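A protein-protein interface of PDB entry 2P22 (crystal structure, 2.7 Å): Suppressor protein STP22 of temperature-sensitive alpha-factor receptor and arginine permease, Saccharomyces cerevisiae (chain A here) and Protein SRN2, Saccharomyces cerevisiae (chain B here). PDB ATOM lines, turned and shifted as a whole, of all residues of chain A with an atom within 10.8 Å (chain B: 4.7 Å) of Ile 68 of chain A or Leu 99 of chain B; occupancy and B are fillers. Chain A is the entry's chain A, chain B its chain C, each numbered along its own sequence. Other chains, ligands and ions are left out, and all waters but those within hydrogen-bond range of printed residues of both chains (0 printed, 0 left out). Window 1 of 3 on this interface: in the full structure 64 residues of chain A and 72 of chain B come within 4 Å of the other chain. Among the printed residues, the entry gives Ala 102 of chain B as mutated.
The side-chain carboxylate (OE1) of Glu 65 of chain A lies within salt-bridge range of the guanidinium group (NH2) of Arg 62 of chain A, at 3.7 Å.
The side-chain amide nitrogen (ND2) of Asn 76 of chain A lies within hydrogen-bond range of the backbone carbonyl oxygen (O) of Met 72 of chain A, 2.9 Å away.
The side-chain amide nitrogen of Asn 101 of chain B sits at hydrogen-bond distance from the backbone carbonyl oxygen of Ala 97 of chain B.
Among the printed residues, merely in contact across the chains: Leu 61 of chain A with Val 95 of chain B (3.7 Å), Glu 65 of chain A with Val 95 of chain B (3.5 Å), Glu 65 of chain A with Leu 98 of chain B (3.1 Å), Ile 68 of chain A with Leu 98 of chain B (3.2 Å), Ile 68 of chain A with Leu 99 of chain B (3.6 Å), Ile 68 of chain A with Ala 102 of chain B (3.5 Å), Met 72 of chain A with Asn 101 of chain B (3.5 Å), Met 72 of chain A with Ala 102 of chain B (3.3 Å) and Leu 75 of chain A with Ala 102 of chain B (3.9 Å).
Of the printed residues of chain B, Ile 68 of chain A touches Leu 98, Leu 99 and Ala 102.
Leu 99 of chain B touches just one residue of chain A: Ile 68.
No residue of chain A comes within 4 Å of Ala 97 of chain B.
Leu 98 of chain B touches just these residues of chain A: Glu 65 and Ile 68.
Asn 101 of chain B touches one residue of chain A.
Printed residues of chain A within 4 Å of Ala 102 of chain B: Ile 68 (3.5 Å), Met 72 (3.3 Å) and Leu 75 (3.9 Å).
No residue of chain A comes within 4 Å of Arg 103 of chain B.
Printed residues of chain B within 4 Å of Leu 75 of chain A: Ala 102 (3.9 Å).
Of the printed residues of chain B, Met 72 of chain A touches Asn 101 (3.5 Å) and Ala 102 (3.3 Å).
Of the printed residues of chain B, Leu 61 of chain A touches Val 95 (3.7 Å).
Printed residues of chain B that touch a printed residue of chain A: Val 95, Leu 98, Leu 99, Asn 101 and Ala 102.
Hydrophobic or aromatic side chains of chain B within 4 Å of the printed part of chain A: Val 95, Leu 98, Leu 99 and Ala 102.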
ATOM      1  N   ASN A  59       6.656  21.105 -11.913  1.00  0.00           N
ATOM      2  CA  ASN A  59       6.562  22.303 -12.758  1.00  0.00           C
ATOM      3  C   ASN A  59       7.890  23.015 -12.839  1.00  0.00           C
ATOM      4  O   ASN A  59       8.355  23.321 -13.928  1.00  0.00           O
ATOM      5  CB  ASN A  59       5.532  23.304 -12.215  1.00  0.00           C
ATOM      6  CG  ASN A  59       4.106  22.799 -12.316  1.00  0.00           C
ATOM      7  OD1 ASN A  59       3.689  22.261 -13.350  1.00  0.00           O
ATOM      8  ND2 ASN A  59       3.339  22.988 -11.244  1.00  0.00           N
ATOM      9  N   HIS A  60       8.489  23.303 -11.684  1.00  0.00           N
ATOM     10  CA  HIS A  60       9.783  23.985 -11.653  1.00  0.00           C
ATOM     11  C   HIS A  60      10.727  23.228 -12.532  1.00  0.00           C
ATOM     12  O   HIS A  60      11.450  23.825 -13.320  1.00  0.00           O
ATOM     13  CB  HIS A  60      10.354  24.041 -10.245  1.00  0.00           C
ATOM     14  CG  HIS A  60       9.839  25.190  -9.437  1.00  0.00           C
ATOM     15  ND1 HIS A  60       8.523  25.599  -9.479  1.00  0.00           N
ATOM     16  CD2 HIS A  60      10.456  26.001  -8.548  1.00  0.00           C
ATOM     17  CE1 HIS A  60       8.351  26.611  -8.649  1.00  0.00           C
ATOM     18  NE2 HIS A  60       9.508  26.875  -8.070  1.00  0.00           N
ATOM     19  N   LEU A  61      10.712  21.907 -12.405  1.00  0.00           N
ATOM     20  CA  LEU A  61      11.581  21.085 -13.216  1.00  0.00           C
ATOM     21  C   LEU A  61      11.333  21.285 -14.701  1.00  0.00           C
ATOM     22  O   LEU A  61      12.284  21.375 -15.468  1.00  0.00           O
ATOM     23  CB  LEU A  61      11.410  19.611 -12.863  1.00  0.00           C
ATOM     24  CG  LEU A  61      12.598  19.044 -12.080  1.00  0.00           C
ATOM     25  CD1 LEU A  61      13.884  19.251 -12.871  1.00  0.00           C
ATOM     26  CD2 LEU A  61      12.693  19.742 -10.739  1.00  0.00           C
ATOM     27  N   ARG A  62      10.069  21.349 -15.116  1.00  0.00           N
ATOM     28  CA  ARG A  62       9.757  21.542 -16.535  1.00  0.00           C
ATOM     29  C   ARG A  62      10.185  22.925 -16.992  1.00  0.00           C
ATOM     30  O   ARG A  62      10.700  23.099 -18.091  1.00  0.00           O
ATOM     31  CB  ARG A  62       8.253  21.380 -16.816  1.00  0.00           C
ATOM     32  CG  ARG A  62       7.714  19.946 -16.839  1.00  0.00           C
ATOM     33  CD  ARG A  62       8.380  19.067 -17.908  1.00  0.00           C
ATOM     34  NE  ARG A  62       9.597  18.409 -17.416  1.00  0.00           N
ATOM     35  CZ  ARG A  62      10.308  17.516 -18.104  1.00  0.00           C
ATOM     36  NH1 ARG A  62       9.931  17.161 -19.328  1.00  0.00           N
ATOM     37  NH2 ARG A  62      11.393  16.973 -17.566  1.00  0.00           N
ATOM     38  N   ALA A  63       9.962  23.915 -16.144  1.00  0.00           N
ATOM     39  CA  ALA A  63      10.324  25.274 -16.481  1.00  0.00           C
ATOM     40  C   ALA A  63      11.812  25.355 -16.790  1.00  0.00           C
ATOM     41  O   ALA A  63      12.203  25.757 -17.884  1.00  0.00           O
ATOM     42  CB  ALA A  63       9.975  26.201 -15.328  1.00  0.00           C
ATOM     43  N   VAL A  64      12.640  24.979 -15.820  1.00  0.00           N
ATOM     44  CA  VAL A  64      14.085  25.029 -16.002  1.00  0.00           C
ATOM     45  C   VAL A  64      14.492  24.156 -17.165  1.00  0.00           C
ATOM     46  O   VAL A  64      15.422  24.480 -17.892  1.00  0.00           O
ATOM     47  CB  VAL A  64      14.844  24.570 -14.735  1.00  0.00           C
ATOM     48  CG1 VAL A  64      14.481  25.470 -13.560  1.00  0.00           C
ATOM     49  CG2 VAL A  64      14.512  23.120 -14.423  1.00  0.00           C
ATOM     50  N   GLU A  65      13.783  23.049 -17.338  1.00  0.00           N
ATOM     51  CA  GLU A  65      14.064  22.125 -18.427  1.00  0.00           C
ATOM     52  C   GLU A  65      14.049  22.876 -19.753  1.00  0.00           C
ATOM     53  O   GLU A  65      15.016  22.835 -20.515  1.00  0.00           O
ATOM     54  CB  GLU A  65      13.007  21.016 -18.451  1.00  0.00           C
ATOM     55  CG  GLU A  65      13.052  20.141 -19.696  1.00  0.00           C
ATOM     56  CD  GLU A  65      14.336  19.348 -19.806  1.00  0.00           C
ATOM     57  OE1 GLU A  65      14.459  18.319 -19.112  1.00  0.00           O
ATOM     58  OE2 GLU A  65      15.229  19.763 -20.575  1.00  0.00           O
ATOM     59  N   GLN A  66      12.937  23.559 -20.014  1.00  0.00           N
ATOM     60  CA  GLN A  66      12.756  24.324 -21.237  1.00  0.00           C
ATOM     61  C   GLN A  66      13.685  25.529 -21.202  1.00  0.00           C
ATOM     62  O   GLN A  66      14.408  25.802 -22.159  1.00  0.00           O
ATOM     63  CB  GLN A  66      11.305  24.795 -21.351  1.00  0.00           C
ATOM     64  CG  GLN A  66      10.260  23.717 -21.070  1.00  0.00           C
ATOM     65  CD  GLN A  66      10.249  22.596 -22.102  1.00  0.00           C
ATOM     66  OE1 GLN A  66      11.262  21.927 -22.330  1.00  0.00           O
ATOM     67  NE2 GLN A  66       9.095  22.386 -22.728  1.00  0.00           N
ATOM     68  N   ALA A  67      13.663  26.241 -20.081  1.00  0.00           N
ATOM     69  CA  ALA A  67      14.494  27.421 -19.910  1.00  0.00           C
ATOM     70  C   ALA A  67      15.944  27.163 -20.319  1.00  0.00           C
ATOM     71  O   ALA A  67      16.547  27.971 -21.019  1.00  0.00           O
ATOM     72  CB  ALA A  67      14.429  27.889 -18.468  1.00  0.00           C
ATOM     73  N   ILE A  68      16.499  26.034 -19.895  1.00  0.00           N
ATOM     74  CA  ILE A  68      17.882  25.708 -20.222  1.00  0.00           C
ATOM     75  C   ILE A  68      18.064  25.344 -21.684  1.00  0.00           C
ATOM     76  O   ILE A  68      19.088  25.667 -22.294  1.00  0.00           O
ATOM     77  CB  ILE A  68      18.406  24.544 -19.368  1.00  0.00           C
ATOM     78  CG1 ILE A  68      18.510  24.991 -17.906  1.00  0.00           C
ATOM     79  CG2 ILE A  68      19.756  24.069 -19.906  1.00  0.00           C
ATOM     80  CD1 ILE A  68      18.887  23.886 -16.940  1.00  0.00           C
ATOM     81  N   GLU A  69      17.084  24.654 -22.248  1.00  0.00           N
ATOM     82  CA  GLU A  69      17.182  24.276 -23.645  1.00  0.00           C
ATOM     83  C   GLU A  69      17.164  25.502 -24.547  1.00  0.00           C
ATOM     84  O   GLU A  69      18.007  25.631 -25.431  1.00  0.00           O
ATOM     85  CB  GLU A  69      16.046  23.336 -24.031  1.00  0.00           C
ATOM     86  CG  GLU A  69      16.251  21.911 -23.584  1.00  0.00           C
ATOM     87  CD  GLU A  69      15.185  20.983 -24.138  1.00  0.00           C
ATOM     88  OE1 GLU A  69      14.019  21.072 -23.686  1.00  0.00           O
ATOM     89  OE2 GLU A  69      15.511  20.172 -25.036  1.00  0.00           O
ATOM     90  N   GLN A  70      16.216  26.409 -24.320  1.00  0.00           N
ATOM     91  CA  GLN A  70      16.128  27.600 -25.154  1.00  0.00           C
ATOM     92  C   GLN A  70      17.383  28.436 -24.978  1.00  0.00           C
ATOM     93  O   GLN A  70      17.944  28.930 -25.951  1.00  0.00           O
ATOM     94  CB  GLN A  70      14.889  28.441 -24.805  1.00  0.00           C
ATOM     95  CG  GLN A  70      14.522  29.468 -25.901  1.00  0.00           C
ATOM     96  CD  GLN A  70      13.281  30.312 -25.584  1.00  0.00           C
ATOM     97  OE1 GLN A  70      13.299  31.166 -24.690  1.00  0.00           O
ATOM     98  NE2 GLN A  70      12.199  30.075 -26.327  1.00  0.00           N
ATOM     99  N   THR A  71      17.832  28.578 -23.738  1.00  0.00           N
ATOM    100  CA  THR A  71      19.026  29.357 -23.462  1.00  0.00           C
ATOM    101  C   THR A  71      20.253  28.742 -24.124  1.00  0.00           C
ATOM    102  O   THR A  71      21.198  29.448 -24.461  1.00  0.00           O
ATOM    103  CB  THR A  71      19.260  29.488 -21.945  1.00  0.00           C
ATOM    104  OG1 THR A  71      18.283  30.380 -21.393  1.00  0.00           O
ATOM    105  CG2 THR A  71      20.655  30.027 -21.653  1.00  0.00           C
ATOM    106  N   MET A  72      20.247  27.430 -24.318  1.00  0.00           N
ATOM    107  CA  MET A  72      21.389  26.798 -24.963  1.00  0.00           C
ATOM    108  C   MET A  72      21.418  27.133 -26.452  1.00  0.00           C
ATOM    109  O   MET A  72      22.486  27.367 -27.017  1.00  0.00           O
ATOM    110  CB  MET A  72      21.354  25.278 -24.783  1.00  0.00           C
ATOM    111  CG  MET A  72      21.837  24.783 -23.432  1.00  0.00           C
ATOM    112  SD  MET A  72      22.362  23.064 -23.534  1.00  0.00           S
ATOM    113  CE  MET A  72      24.100  23.236 -23.870  1.00  0.00           C
ATOM    114  N   HIS A  73      20.247  27.161 -27.087  1.00  0.00           N
ATOM    115  CA  HIS A  73      20.172  27.468 -28.509  1.00  0.00           C
ATOM    116  C   HIS A  73      20.580  28.928 -28.727  1.00  0.00           C
ATOM    117  O   HIS A  73      21.075  29.294 -29.791  1.00  0.00           O
ATOM    118  CB  HIS A  73      18.752  27.226 -29.048  1.00  0.00           C
ATOM    119  CG  HIS A  73      18.716  26.814 -30.491  1.00  0.00           C
ATOM    120  ND1 HIS A  73      19.194  25.597 -30.932  1.00  0.00           N
ATOM    121  CD2 HIS A  73      18.287  27.469 -31.596  1.00  0.00           C
ATOM    122  CE1 HIS A  73      19.063  25.522 -32.245  1.00  0.00           C
ATOM    123  NE2 HIS A  73      18.516  26.646 -32.673  1.00  0.00           N
ATOM    124  N   SER A  74      20.381  29.756 -27.709  1.00  0.00           N
ATOM    125  CA  SER A  74      20.745  31.161 -27.805  1.00  0.00           C
ATOM    126  C   SER A  74      22.253  31.304 -27.774  1.00  0.00           C
ATOM    127  O   SER A  74      22.822  32.204 -28.390  1.00  0.00           O
ATOM    128  CB  SER A  74      20.136  31.954 -26.651  1.00  0.00           C
ATOM    129  OG  SER A  74      18.727  31.982 -26.753  1.00  0.00           O
ATOM    130  N   LEU A  75      22.904  30.408 -27.049  1.00  0.00           N
ATOM    131  CA  LEU A  75      24.346  30.452 -26.950  1.00  0.00           C
ATOM    132  C   LEU A  75      25.003  29.935 -28.220  1.00  0.00           C
ATOM    133  O   LEU A  75      25.865  30.601 -28.788  1.00  0.00           O
ATOM    134  CB  LEU A  75      24.812  29.630 -25.752  1.00  0.00           C
ATOM    135  CG  LEU A  75      24.341  30.153 -24.398  1.00  0.00           C
ATOM    136  CD1 LEU A  75      24.748  29.162 -23.329  1.00  0.00           C
ATOM    137  CD2 LEU A  75      24.930  31.530 -24.120  1.00  0.00           C
ATOM    138  N   ASN A  76      24.593  28.755 -28.675  1.00  0.00           N
ATOM    139  CA  ASN A  76      25.190  28.191 -29.878  1.00  0.00           C
ATOM    140  C   ASN A  76      24.860  29.035 -31.104  1.00  0.00           C
ATOM    141  O   ASN A  76      25.363  28.786 -32.201  1.00  0.00           O
ATOM    142  CB  ASN A  76      24.734  26.742 -30.091  1.00  0.00           C
ATOM    143  CG  ASN A  76      23.246  26.627 -30.333  1.00  0.00           C
ATOM    144  OD1 ASN A  76      22.702  27.237 -31.258  1.00  0.00           O
ATOM    145  ND2 ASN A  76      22.575  25.834 -29.505  1.00  0.00           N
ATOM    146  N   VAL B  95      18.329  16.762 -15.957  1.00  0.00           N
ATOM    147  CA  VAL B  95      18.369  18.213 -15.980  1.00  0.00           C
ATOM    148  C   VAL B  95      19.657  18.693 -15.328  1.00  0.00           C
ATOM    149  O   VAL B  95      20.212  19.723 -15.706  1.00  0.00           O
ATOM    150  CB  VAL B  95      17.175  18.807 -15.215  1.00  0.00           C
ATOM    151  CG1 VAL B  95      17.307  20.322 -15.118  1.00  0.00           C
ATOM    152  CG2 VAL B  95      15.880  18.426 -15.909  1.00  0.00           C
ATOM    153  N   GLN B  96      20.133  17.937 -14.345  1.00  0.00           N
ATOM    154  CA  GLN B  96      21.358  18.290 -13.633  1.00  0.00           C
ATOM    155  C   GLN B  96      22.564  18.108 -14.566  1.00  0.00           C
ATOM    156  O   GLN B  96      23.668  18.582 -14.279  1.00  0.00           O
ATOM    157  CB  GLN B  96      21.481  17.419 -12.369  1.00  0.00           C
ATOM    158  CG  GLN B  96      22.397  17.974 -11.275  1.00  0.00           C
ATOM    159  CD  GLN B  96      21.936  17.610  -9.855  1.00  0.00           C
ATOM    160  OE1 GLN B  96      21.710  16.437  -9.532  1.00  0.00           O
ATOM    161  NE2 GLN B  96      21.807  18.625  -9.000  1.00  0.00           N
ATOM    162  N   ALA B  97      22.326  17.438 -15.696  1.00  0.00           N
ATOM    163  CA  ALA B  97      23.357  17.177 -16.698  1.00  0.00           C
ATOM    164  C   ALA B  97      23.196  18.113 -17.897  1.00  0.00           C
ATOM    165  O   ALA B  97      24.175  18.630 -18.440  1.00  0.00           O
ATOM    166  CB  ALA B  97      23.284  15.732 -17.150  1.00  0.00           C
ATOM    167  N   LEU B  98      21.953  18.326 -18.307  1.00  0.00           N
ATOM    168  CA  LEU B  98      21.660  19.215 -19.425  1.00  0.00           C
ATOM    169  C   LEU B  98      22.055  20.629 -18.994  1.00  0.00           C
ATOM    170  O   LEU B  98      22.340  21.486 -19.824  1.00  0.00           O
ATOM    171  CB  LEU B  98      20.169  19.141 -19.756  1.00  0.00           C
ATOM    172  CG  LEU B  98      19.652  19.649 -21.099  1.00  0.00           C
ATOM    173  CD1 LEU B  98      18.224  19.157 -21.301  1.00  0.00           C
ATOM    174  CD2 LEU B  98      19.709  21.160 -21.149  1.00  0.00           C
ATOM    175  N   LEU B  99      22.071  20.852 -17.683  1.00  0.00           N
ATOM    176  CA  LEU B  99      22.455  22.134 -17.124  1.00  0.00           C
ATOM    177  C   LEU B  99      23.960  22.138 -17.047  1.00  0.00           C
ATOM    178  O   LEU B  99      24.593  23.189 -17.059  1.00  0.00           O
ATOM    179  CB  LEU B  99      21.871  22.311 -15.727  1.00  0.00           C
ATOM    180  CG  LEU B  99      22.323  23.528 -14.916  1.00  0.00           C
ATOM    181  CD1 LEU B  99      21.237  23.863 -13.913  1.00  0.00           C
ATOM    182  CD2 LEU B  99      23.650  23.264 -14.200  1.00  0.00           C
ATOM    183  N   GLU B 100      24.538  20.949 -16.966  1.00  0.00           N
ATOM    184  CA  GLU B 100      25.984  20.837 -16.894  1.00  0.00           C
ATOM    185  C   GLU B 100      26.569  21.233 -18.246  1.00  0.00           C
ATOM    186  O   GLU B 100      27.738  21.595 -18.337  1.00  0.00           O
ATOM    187  CB  GLU B 100      26.378  19.403 -16.511  1.00  0.00           C
ATOM    188  CG  GLU B 100      27.875  19.163 -16.369  1.00  0.00           C
ATOM    189  CD  GLU B 100      28.548  18.872 -17.697  1.00  0.00           C
ATOM    190  OE1 GLU B 100      28.131  17.910 -18.378  1.00  0.00           O
ATOM    191  OE2 GLU B 100      29.495  19.601 -18.062  1.00  0.00           O
ATOM    192  N   ASN B 101      25.749  21.179 -19.294  1.00  0.00           N
ATOM    193  CA  ASN B 101      26.204  21.554 -20.632  1.00  0.00           C
ATOM    194  C   ASN B 101      25.965  23.029 -20.911  1.00  0.00           C
ATOM    195  O   ASN B 101      26.831  23.707 -21.455  1.00  0.00           O
ATOM    196  CB  ASN B 101      25.505  20.716 -21.699  1.00  0.00           C
ATOM    197  CG  ASN B 101      25.991  19.283 -21.721  1.00  0.00           C
ATOM    198  OD1 ASN B 101      27.180  19.019 -21.915  1.00  0.00           O
ATOM    199  ND2 ASN B 101      25.073  18.347 -21.521  1.00  0.00           N
ATOM    200  N   ALA B 102      24.789  23.526 -20.546  1.00  0.00           N
ATOM    201  CA  ALA B 102      24.494  24.931 -20.765  1.00  0.00           C
ATOM    202  C   ALA B 102      25.452  25.793 -19.945  1.00  0.00           C
ATOM    203  O   ALA B 102      25.501  27.010 -20.115  1.00  0.00           O
ATOM    204  CB  ALA B 102      23.055  25.239 -20.389  1.00  0.00           C
ATOM    205  N   ARG B 103      26.217  25.171 -19.054  1.00  0.00           N
ATOM    206  CA  ARG B 103      27.165  25.928 -18.245  1.00  0.00           C
ATOM    207  C   ARG B 103      28.551  25.908 -18.869  1.00  0.00           C
ATOM    208  O   ARG B 103      29.326  26.856 -18.713  1.00  0.00           O
ATOM    209  CB  ARG B 103      27.245  25.369 -16.826  1.00  0.00           C
ATOM    210  CG  ARG B 103      26.267  25.982 -15.845  1.00  0.00           C
ATOM    211  CD  ARG B 103      26.405  25.306 -14.492  1.00  0.00           C
ATOM    212  NE  ARG B 103      25.648  25.996 -13.454  1.00  0.00           N
ATOM    213  CZ  ARG B 103      25.650  25.650 -12.171  1.00  0.00           C
ATOM    214  NH1 ARG B 103      26.367  24.614 -11.757  1.00  0.00           N
ATOM    215  NH2 ARG B 103      24.939  26.350 -11.295  1.00  0.00           N
